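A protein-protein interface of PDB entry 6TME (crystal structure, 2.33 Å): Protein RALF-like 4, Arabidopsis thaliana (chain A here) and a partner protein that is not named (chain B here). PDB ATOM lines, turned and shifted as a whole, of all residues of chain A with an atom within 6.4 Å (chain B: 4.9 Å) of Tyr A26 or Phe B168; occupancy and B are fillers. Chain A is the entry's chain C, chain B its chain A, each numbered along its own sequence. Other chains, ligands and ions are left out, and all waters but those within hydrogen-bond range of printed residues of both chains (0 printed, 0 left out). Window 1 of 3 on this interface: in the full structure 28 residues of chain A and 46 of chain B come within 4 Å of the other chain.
Hydrophobic or aromatic side chains of chain B within 4 Å of the printed part of chain A: His B122, Tyr B143, Phe B168, Ala B191 and Phe B193. Among the printed residues, 14 pairs touch across the chains. Among the printed residues, no Asp or Glu carboxylate lies within 4 Å of a Lys or Arg side-chain nitrogen of the other chain.
Of chain B, only Asn B100, His B122, Glu B144, Asp B146 and Phe B168 come within 4 Å of Tyr A26. Of the printed residues of chain A, Phe B168 touches Tyr A26 (3.7 Å) and Tyr A27 (3.5 Å). Of the printed residues of chain A, Ala B191 touches Ile A45. Of the printed residues of chain A, Phe B193 touches Ile A7. Of the printed residues of chain B, Tyr A27 touches Tyr B143, Lys B167 and Phe B168. Printed residues of chain A within 4 Å of Asn B100: Val A17 and Tyr A26. The nearest residue of chain A that does not touch Phe B168 is Pro A18 (4.2 Å).
N of Phe B145 is in hydrogen-bond range of O of Phe B168 (2.9 Å). O of Tyr B143 sits at hydrogen-bond distance from N of Phe B168, 3.0 Å away. A ring nitrogen (NE2) of His B122 is in hydrogen-bond range of the side-chain carboxylate of Glu B144, at 2.6 Å. The side-chain hydroxyl (OG) of Ser A25 sits close to the backbone NH (N) of Tyr A27 (3.0 Å). O of Tyr B143 lies within hydrogen-bond range of N of Lys B167 (2.8 Å). OD1 of Asn B100 lies close to O of His B122 (3.5 Å).
Ile A7 touches Phe B193 (CG1 to CZ, 3.96 Å). Val A17 touches Asn B100 (CG1 to ND2, 3.8 Å). O of Arg A24 touches CE1 of His B122, 3.3 Å away. Tyr A26 touches Phe B168. Tyr A27 touches Tyr B143. Tyr A27 touches Lys B167 (OH to CG, 3.6 Å). CD2 of Phe B168 touches OH of Tyr A27 (3.5 Å). Lys B167 touches Cys A42 (NZ to O, 3.5 Å). Ile A45 touches Ala B191.
OH of Tyr A26 sits at hydrogen-bond distance from ND2 of Asn B100 (3.0 Å). OG of Ser A25 lies close to OE2 of Glu B144 (2.4 Å). OE1 of Glu B144 sits at hydrogen-bond distance from N of Tyr A26, 3.0 Å away. The side-chain hydroxyl of Tyr A26 is in hydrogen-bond range of the side-chain carboxylate of Asp B146 (2.9 Å). A ring nitrogen (ND1) of His B122 sits close to the side-chain hydroxyl (OH) of Tyr A26 (3.5 Å).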
ATOM      1  N   ILE A   7       2.409 -35.240   4.851  1.00  0.00           N
ATOM      2  CA  ILE A   7       2.484 -33.797   4.720  1.00  0.00           C
ATOM      3  C   ILE A   7       1.859 -33.349   3.404  1.00  0.00           C
ATOM      4  O   ILE A   7       1.399 -32.204   3.286  1.00  0.00           O
ATOM      5  CB  ILE A   7       3.942 -33.324   4.862  1.00  0.00           C
ATOM      6  CG1 ILE A   7       4.007 -31.781   4.871  1.00  0.00           C
ATOM      7  CG2 ILE A   7       4.780 -33.926   3.759  1.00  0.00           C
ATOM      8  CD1 ILE A   7       5.331 -31.225   5.261  1.00  0.00           C
ATOM      9  N   VAL A  17       1.223 -26.069   9.387  1.00  0.00           N
ATOM     10  CA  VAL A  17       2.633 -25.898   9.038  1.00  0.00           C
ATOM     11  C   VAL A  17       3.391 -27.084   9.609  1.00  0.00           C
ATOM     12  O   VAL A  17       2.893 -27.762  10.518  1.00  0.00           O
ATOM     13  CB  VAL A  17       3.199 -24.557   9.574  1.00  0.00           C
ATOM     14  CG1 VAL A  17       2.596 -23.408   8.842  1.00  0.00           C
ATOM     15  CG2 VAL A  17       2.939 -24.416  11.075  1.00  0.00           C
ATOM     16  N   PRO A  18       4.594 -27.374   9.101  1.00  0.00           N
ATOM     17  CA  PRO A  18       5.308 -28.578   9.570  1.00  0.00           C
ATOM     18  C   PRO A  18       5.814 -28.472  10.991  1.00  0.00           C
ATOM     19  O   PRO A  18       6.122 -29.505  11.601  1.00  0.00           O
ATOM     20  CB  PRO A  18       6.469 -28.712   8.574  1.00  0.00           C
ATOM     21  CG  PRO A  18       6.027 -27.923   7.357  1.00  0.00           C
ATOM     22  CD  PRO A  18       5.269 -26.765   7.936  1.00  0.00           C
ATOM     23  N   CYS A  19       5.888 -27.265  11.552  1.00  0.00           N
ATOM     24  CA  CYS A  19       6.538 -27.076  12.841  1.00  0.00           C
ATOM     25  C   CYS A  19       5.912 -25.893  13.567  1.00  0.00           C
ATOM     26  O   CYS A  19       5.766 -24.807  13.000  1.00  0.00           O
ATOM     27  CB  CYS A  19       8.045 -26.849  12.661  1.00  0.00           C
ATOM     28  SG  CYS A  19       8.941 -26.537  14.175  1.00  0.00           S
ATOM     29  N   SER A  20       5.568 -26.106  14.825  1.00  0.00           N
ATOM     30  CA  SER A  20       4.948 -25.081  15.644  1.00  0.00           C
ATOM     31  C   SER A  20       5.951 -24.231  16.422  1.00  0.00           C
ATOM     32  O   SER A  20       5.543 -23.251  17.052  1.00  0.00           O
ATOM     33  CB  SER A  20       3.963 -25.735  16.611  1.00  0.00           C
ATOM     34  OG  SER A  20       4.626 -26.690  17.422  1.00  0.00           O
ATOM     35  N   ARG A  24      12.265 -22.056  14.172  1.00  0.00           N
ATOM     36  CA  ARG A  24      12.995 -23.273  13.861  1.00  0.00           C
ATOM     37  C   ARG A  24      12.788 -23.693  12.416  1.00  0.00           C
ATOM     38  O   ARG A  24      11.715 -23.497  11.836  1.00  0.00           O
ATOM     39  CB  ARG A  24      12.557 -24.413  14.781  1.00  0.00           C
ATOM     40  CG  ARG A  24      13.073 -24.217  16.182  1.00  0.00           C
ATOM     41  CD  ARG A  24      13.056 -25.479  16.987  1.00  0.00           C
ATOM     42  NE  ARG A  24      13.332 -25.126  18.365  1.00  0.00           N
ATOM     43  CZ  ARG A  24      14.552 -24.892  18.828  1.00  0.00           C
ATOM     44  NH1 ARG A  24      15.599 -25.009  18.018  1.00  0.00           N
ATOM     45  NH2 ARG A  24      14.723 -24.552  20.101  1.00  0.00           N
ATOM     46  N   SER A  25      13.821 -24.302  11.845  1.00  0.00           N
ATOM     47  CA  SER A  25      13.680 -24.886  10.518  1.00  0.00           C
ATOM     48  C   SER A  25      12.631 -25.989  10.536  1.00  0.00           C
ATOM     49  O   SER A  25      12.520 -26.756  11.507  1.00  0.00           O
ATOM     50  CB  SER A  25      15.004 -25.449  10.028  1.00  0.00           C
ATOM     51  OG  SER A  25      14.850 -26.054   8.763  1.00  0.00           O
ATOM     52  N   TYR A  26      11.843 -26.057   9.454  1.00  0.00           N
ATOM     53  CA  TYR A  26      10.970 -27.203   9.234  1.00  0.00           C
ATOM     54  C   TYR A  26      11.761 -28.512   9.179  1.00  0.00           C
ATOM     55  O   TYR A  26      11.188 -29.592   9.345  1.00  0.00           O
ATOM     56  CB  TYR A  26      10.179 -26.974   7.949  1.00  0.00           C
ATOM     57  CG  TYR A  26       9.190 -25.833   8.041  1.00  0.00           C
ATOM     58  CD1 TYR A  26       8.762 -25.353   9.279  1.00  0.00           C
ATOM     59  CD2 TYR A  26       8.691 -25.236   6.902  1.00  0.00           C
ATOM     60  CE1 TYR A  26       7.857 -24.317   9.371  1.00  0.00           C
ATOM     61  CE2 TYR A  26       7.785 -24.188   6.982  1.00  0.00           C
ATOM     62  CZ  TYR A  26       7.372 -23.738   8.209  1.00  0.00           C
ATOM     63  OH  TYR A  26       6.469 -22.707   8.269  1.00  0.00           O
ATOM     64  N   TYR A  27      13.069 -28.432   8.964  1.00  0.00           N
ATOM     65  CA  TYR A  27      13.940 -29.590   8.932  1.00  0.00           C
ATOM     66  C   TYR A  27      14.631 -29.855  10.262  1.00  0.00           C
ATOM     67  O   TYR A  27      15.542 -30.685  10.318  1.00  0.00           O
ATOM     68  CB  TYR A  27      14.968 -29.408   7.817  1.00  0.00           C
ATOM     69  CG  TYR A  27      14.300 -29.417   6.473  1.00  0.00           C
ATOM     70  CD1 TYR A  27      14.101 -30.610   5.786  1.00  0.00           C
ATOM     71  CD2 TYR A  27      13.802 -28.247   5.923  1.00  0.00           C
ATOM     72  CE1 TYR A  27      13.459 -30.625   4.550  1.00  0.00           C
ATOM     73  CE2 TYR A  27      13.162 -28.245   4.702  1.00  0.00           C
ATOM     74  CZ  TYR A  27      12.996 -29.440   4.018  1.00  0.00           C
ATOM     75  OH  TYR A  27      12.345 -29.451   2.809  1.00  0.00           O
ATOM     76  N   ASP A  28      14.217 -29.185  11.333  1.00  0.00           N
ATOM     77  CA  ASP A  28      14.831 -29.381  12.644  1.00  0.00           C
ATOM     78  C   ASP A  28      13.838 -28.979  13.732  1.00  0.00           C
ATOM     79  O   ASP A  28      14.135 -28.142  14.586  1.00  0.00           O
ATOM     80  CB  ASP A  28      16.136 -28.584  12.752  1.00  0.00           C
ATOM     81  CG  ASP A  28      16.888 -28.845  14.063  1.00  0.00           C
ATOM     82  OD1 ASP A  28      17.208 -30.018  14.329  1.00  0.00           O
ATOM     83  OD2 ASP A  28      17.170 -27.887  14.825  1.00  0.00           O
ATOM     84  N   CYS A  29      12.638 -29.552  13.708  1.00  0.00           N
ATOM     85  CA  CYS A  29      11.648 -29.229  14.728  1.00  0.00           C
ATOM     86  C   CYS A  29      11.913 -30.137  15.924  1.00  0.00           C
ATOM     87  O   CYS A  29      11.302 -31.191  16.113  1.00  0.00           O
ATOM     88  CB  CYS A  29      10.241 -29.374  14.173  1.00  0.00           C
ATOM     89  SG  CYS A  29       8.999 -28.394  15.054  1.00  0.00           S
ATOM     90  N   CYS A  42      17.259 -33.018   9.165  1.00  0.00           N
ATOM     91  CA  CYS A  42      16.386 -33.904   8.410  1.00  0.00           C
ATOM     92  C   CYS A  42      16.622 -33.704   6.916  1.00  0.00           C
ATOM     93  O   CYS A  42      16.861 -32.583   6.448  1.00  0.00           O
ATOM     94  CB  CYS A  42      14.923 -33.645   8.784  1.00  0.00           C
ATOM     95  SG  CYS A  42      13.674 -34.100   7.524  1.00  0.00           S
ATOM     96  N   ILE A  45      11.542 -33.880   3.943  1.00  0.00           N
ATOM     97  CA  ILE A  45      10.508 -33.389   4.846  1.00  0.00           C
ATOM     98  C   ILE A  45       9.438 -34.458   5.093  1.00  0.00           C
ATOM     99  O   ILE A  45       8.893 -34.547   6.202  1.00  0.00           O
ATOM    100  CB  ILE A  45       9.920 -32.069   4.290  1.00  0.00           C
ATOM    101  CG1 ILE A  45       8.934 -31.432   5.276  1.00  0.00           C
ATOM    102  CG2 ILE A  45       9.213 -32.316   2.972  1.00  0.00           C
ATOM    103  CD1 ILE A  45       9.575 -30.737   6.422  1.00  0.00           C
ATOM    104  N   CYS A  48      10.685 -36.635   8.114  1.00  0.00           N
ATOM    105  CA  CYS A  48      10.672 -36.076   9.462  1.00  0.00           C
ATOM    106  C   CYS A  48       9.332 -35.462   9.845  1.00  0.00           C
ATOM    107  O   CYS A  48       9.123 -35.160  11.024  1.00  0.00           O
ATOM    108  CB  CYS A  48      11.786 -35.039   9.644  1.00  0.00           C
ATOM    109  SG  CYS A  48      11.866 -33.737   8.402  1.00  0.00           S
ATOM    110  N   TYR A  49       8.428 -35.264   8.886  1.00  0.00           N
ATOM    111  CA  TYR A  49       7.037 -35.009   9.235  1.00  0.00           C
ATOM    112  C   TYR A  49       6.406 -36.220   9.893  1.00  0.00           C
ATOM    113  O   TYR A  49       5.562 -36.061  10.778  1.00  0.00           O
ATOM    114  CB  TYR A  49       6.227 -34.654   7.992  1.00  0.00           C
ATOM    115  CG  TYR A  49       4.914 -33.970   8.292  1.00  0.00           C
ATOM    116  CD1 TYR A  49       4.889 -32.663   8.773  1.00  0.00           C
ATOM    117  CD2 TYR A  49       3.703 -34.622   8.094  1.00  0.00           C
ATOM    118  CE1 TYR A  49       3.710 -32.030   9.043  1.00  0.00           C
ATOM    119  CE2 TYR A  49       2.507 -33.991   8.362  1.00  0.00           C
ATOM    120  CZ  TYR A  49       2.522 -32.685   8.835  1.00  0.00           C
ATOM    121  OH  TYR A  49       1.350 -32.021   9.097  1.00  0.00           O
ATOM    122  N   ASN B 100       4.451 -16.920  11.378  1.00  0.00           N
ATOM    123  CA  ASN B 100       3.364 -17.865  11.134  1.00  0.00           C
ATOM    124  C   ASN B 100       2.168 -17.553  12.015  1.00  0.00           C
ATOM    125  O   ASN B 100       2.305 -17.376  13.228  1.00  0.00           O
ATOM    126  CB  ASN B 100       3.814 -19.310  11.378  1.00  0.00           C
ATOM    127  CG  ASN B 100       4.597 -19.873  10.233  1.00  0.00           C
ATOM    128  OD1 ASN B 100       4.701 -19.259   9.170  1.00  0.00           O
ATOM    129  ND2 ASN B 100       5.170 -21.041  10.438  1.00  0.00           N
ATOM    130  N   HIS B 122       9.214 -17.760   7.222  1.00  0.00           N
ATOM    131  CA  HIS B 122       7.922 -18.401   7.467  1.00  0.00           C
ATOM    132  C   HIS B 122       6.879 -17.318   7.728  1.00  0.00           C
ATOM    133  O   HIS B 122       6.945 -16.639   8.757  1.00  0.00           O
ATOM    134  CB  HIS B 122       7.993 -19.359   8.662  1.00  0.00           C
ATOM    135  CG  HIS B 122       8.986 -20.473   8.504  1.00  0.00           C
ATOM    136  ND1 HIS B 122       9.361 -21.284   9.555  1.00  0.00           N
ATOM    137  CD2 HIS B 122       9.683 -20.910   7.426  1.00  0.00           C
ATOM    138  CE1 HIS B 122      10.256 -22.163   9.135  1.00  0.00           C
ATOM    139  NE2 HIS B 122      10.475 -21.952   7.848  1.00  0.00           N
ATOM    140  N   TYR B 143      16.669 -20.820   1.923  1.00  0.00           N
ATOM    141  CA  TYR B 143      16.615 -22.266   2.034  1.00  0.00           C
ATOM    142  C   TYR B 143      15.190 -22.783   2.158  1.00  0.00           C
ATOM    143  O   TYR B 143      14.844 -23.778   1.513  1.00  0.00           O
ATOM    144  CB  TYR B 143      17.452 -22.682   3.252  1.00  0.00           C
ATOM    145  CG  TYR B 143      17.593 -24.170   3.561  1.00  0.00           C
ATOM    146  CD1 TYR B 143      18.674 -24.907   3.075  1.00  0.00           C
ATOM    147  CD2 TYR B 143      16.705 -24.803   4.415  1.00  0.00           C
ATOM    148  CE1 TYR B 143      18.832 -26.240   3.386  1.00  0.00           C
ATOM    149  CE2 TYR B 143      16.845 -26.130   4.728  1.00  0.00           C
ATOM    150  CZ  TYR B 143      17.912 -26.847   4.217  1.00  0.00           C
ATOM    151  OH  TYR B 143      18.050 -28.172   4.564  1.00  0.00           O
ATOM    152  N   GLU B 144      14.354 -22.108   2.957  1.00  0.00           N
ATOM    153  CA  GLU B 144      12.957 -22.478   3.174  1.00  0.00           C
ATOM    154  C   GLU B 144      12.111 -21.215   3.151  1.00  0.00           C
ATOM    155  O   GLU B 144      12.248 -20.344   4.017  1.00  0.00           O
ATOM    156  CB  GLU B 144      12.726 -23.235   4.493  1.00  0.00           C
ATOM    157  CG  GLU B 144      13.450 -22.716   5.713  1.00  0.00           C
ATOM    158  CD  GLU B 144      13.330 -23.656   6.919  1.00  0.00           C
ATOM    159  OE1 GLU B 144      12.226 -23.796   7.498  1.00  0.00           O
ATOM    160  OE2 GLU B 144      14.360 -24.271   7.269  1.00  0.00           O
ATOM    161  N   PHE B 145      11.202 -21.157   2.188  1.00  0.00           N
ATOM    162  CA  PHE B 145      10.384 -19.992   1.907  1.00  0.00           C
ATOM    163  C   PHE B 145       8.941 -20.449   1.955  1.00  0.00           C
ATOM    164  O   PHE B 145       8.523 -21.274   1.137  1.00  0.00           O
ATOM    165  CB  PHE B 145      10.725 -19.420   0.530  1.00  0.00           C
ATOM    166  CG  PHE B 145      10.223 -18.044   0.308  1.00  0.00           C
ATOM    167  CD1 PHE B 145      10.858 -16.949   0.909  1.00  0.00           C
ATOM    168  CD2 PHE B 145       9.142 -17.821  -0.547  1.00  0.00           C
ATOM    169  CE1 PHE B 145      10.393 -15.651   0.686  1.00  0.00           C
ATOM    170  CE2 PHE B 145       8.667 -16.528  -0.775  1.00  0.00           C
ATOM    171  CZ  PHE B 145       9.286 -15.442  -0.158  1.00  0.00           C
ATOM    172  N   ASP B 146       8.189 -19.941   2.915  1.00  0.00           N
ATOM    173  CA  ASP B 146       6.828 -20.409   3.142  1.00  0.00           C
ATOM    174  C   ASP B 146       5.957 -19.164   3.180  1.00  0.00           C
ATOM    175  O   ASP B 146       5.927 -18.456   4.195  1.00  0.00           O
ATOM    176  CB  ASP B 146       6.721 -21.224   4.431  1.00  0.00           C
ATOM    177  CG  ASP B 146       5.294 -21.730   4.703  1.00  0.00           C
ATOM    178  OD1 ASP B 146       4.419 -21.621   3.807  1.00  0.00           O
ATOM    179  OD2 ASP B 146       5.052 -22.229   5.829  1.00  0.00           O
ATOM    180  N   LEU B 166      17.911 -23.118  -2.233  1.00  0.00           N
ATOM    181  CA  LEU B 166      16.502 -23.303  -1.930  1.00  0.00           C
ATOM    182  C   LEU B 166      16.117 -24.789  -1.872  1.00  0.00           C
ATOM    183  O   LEU B 166      16.399 -25.567  -2.790  1.00  0.00           O
ATOM    184  CB  LEU B 166      15.668 -22.574  -2.970  1.00  0.00           C
ATOM    185  CG  LEU B 166      14.160 -22.768  -2.795  1.00  0.00           C
ATOM    186  CD1 LEU B 166      13.726 -22.207  -1.479  1.00  0.00           C
ATOM    187  CD2 LEU B 166      13.390 -22.126  -3.930  1.00  0.00           C
ATOM    188  N   LYS B 167      15.463 -25.171  -0.788  1.00  0.00           N
ATOM    189  CA  LYS B 167      15.088 -26.542  -0.511  1.00  0.00           C
ATOM    190  C   LYS B 167      13.590 -26.732  -0.300  1.00  0.00           C
ATOM    191  O   LYS B 167      13.063 -27.798  -0.616  1.00  0.00           O
ATOM    192  CB  LYS B 167      15.828 -27.050   0.741  1.00  0.00           C
ATOM    193  CG  LYS B 167      15.426 -28.468   1.132  1.00  0.00           C
ATOM    194  CD  LYS B 167      16.332 -29.080   2.147  1.00  0.00           C
ATOM    195  CE  LYS B 167      16.314 -30.598   2.034  1.00  0.00           C
ATOM    196  NZ  LYS B 167      16.997 -31.227   3.185  1.00  0.00           N
ATOM    197  N   PHE B 168      12.898 -25.724   0.215  1.00  0.00           N
ATOM    198  CA  PHE B 168      11.503 -25.816   0.615  1.00  0.00           C
ATOM    199  C   PHE B 168      10.820 -24.574   0.080  1.00  0.00           C
ATOM    200  O   PHE B 168      11.199 -23.450   0.442  1.00  0.00           O
ATOM    201  CB  PHE B 168      11.382 -25.899   2.136  1.00  0.00           C
ATOM    202  CG  PHE B 168       9.976 -26.098   2.650  1.00  0.00           C
ATOM    203  CD1 PHE B 168       9.065 -25.046   2.697  1.00  0.00           C
ATOM    204  CD2 PHE B 168       9.585 -27.335   3.143  1.00  0.00           C
ATOM    205  CE1 PHE B 168       7.798 -25.246   3.210  1.00  0.00           C
ATOM    206  CE2 PHE B 168       8.341 -27.528   3.649  1.00  0.00           C
ATOM    207  CZ  PHE B 168       7.449 -26.495   3.690  1.00  0.00           C
ATOM    208  N   LEU B 169       9.844 -24.775  -0.797  1.00  0.00           N
ATOM    209  CA  LEU B 169       9.071 -23.696  -1.394  1.00  0.00           C
ATOM    210  C   LEU B 169       7.606 -24.012  -1.162  1.00  0.00           C
ATOM    211  O   LEU B 169       7.095 -24.996  -1.709  1.00  0.00           O
ATOM    212  CB  LEU B 169       9.379 -23.572  -2.878  1.00  0.00           C
ATOM    213  CG  LEU B 169       8.688 -22.445  -3.653  1.00  0.00           C
ATOM    214  CD1 LEU B 169       8.850 -21.115  -2.967  1.00  0.00           C
ATOM    215  CD2 LEU B 169       9.227 -22.366  -5.084  1.00  0.00           C
ATOM    216  N   ASP B 170       6.932 -23.192  -0.348  1.00  0.00           N
ATOM    217  CA  ASP B 170       5.489 -23.305  -0.132  1.00  0.00           C
ATOM    218  C   ASP B 170       4.778 -22.015  -0.545  1.00  0.00           C
ATOM    219  O   ASP B 170       4.869 -21.004   0.152  1.00  0.00           O
ATOM    220  CB  ASP B 170       5.181 -23.647   1.323  1.00  0.00           C
ATOM    221  CG  ASP B 170       3.748 -24.149   1.509  1.00  0.00           C
ATOM    222  OD1 ASP B 170       2.901 -23.812   0.655  1.00  0.00           O
ATOM    223  OD2 ASP B 170       3.460 -24.864   2.500  1.00  0.00           O
ATOM    224  N   LEU B 189      14.907 -28.776  -5.129  1.00  0.00           N
ATOM    225  CA  LEU B 189      13.917 -28.656  -4.072  1.00  0.00           C
ATOM    226  C   LEU B 189      13.614 -30.026  -3.478  1.00  0.00           C
ATOM    227  O   LEU B 189      13.577 -31.041  -4.184  1.00  0.00           O
ATOM    228  CB  LEU B 189      12.635 -28.015  -4.621  1.00  0.00           C
ATOM    229  CG  LEU B 189      12.752 -26.506  -4.846  1.00  0.00           C
ATOM    230  CD1 LEU B 189      11.652 -26.029  -5.752  1.00  0.00           C
ATOM    231  CD2 LEU B 189      12.644 -25.807  -3.510  1.00  0.00           C
ATOM    232  N   ALA B 191      10.796 -30.058  -1.468  1.00  0.00           N
ATOM    233  CA  ALA B 191       9.361 -29.944  -1.246  1.00  0.00           C
ATOM    234  C   ALA B 191       8.834 -28.768  -2.053  1.00  0.00           C
ATOM    235  O   ALA B 191       9.381 -27.663  -1.969  1.00  0.00           O
ATOM    236  CB  ALA B 191       9.039 -29.752   0.240  1.00  0.00           C
ATOM    237  N   PHE B 193       5.107 -27.084  -2.777  1.00  0.00           N
ATOM    238  CA  PHE B 193       3.672 -26.999  -2.519  1.00  0.00           C
ATOM    239  C   PHE B 193       3.099 -25.901  -3.407  1.00  0.00           C
ATOM    240  O   PHE B 193       3.440 -24.728  -3.244  1.00  0.00           O
ATOM    241  CB  PHE B 193       3.392 -26.731  -1.037  1.00  0.00           C
ATOM    242  CG  PHE B 193       3.922 -27.810  -0.123  1.00  0.00           C
ATOM    243  CD1 PHE B 193       3.241 -28.997   0.025  1.00  0.00           C
ATOM    244  CD2 PHE B 193       5.128 -27.640   0.566  1.00  0.00           C
ATOM    245  CE1 PHE B 193       3.725 -30.007   0.862  1.00  0.00           C
ATOM    246  CE2 PHE B 193       5.627 -28.643   1.395  1.00  0.00           C
ATOM    247  CZ  PHE B 193       4.919 -29.829   1.548  1.00  0.00           C
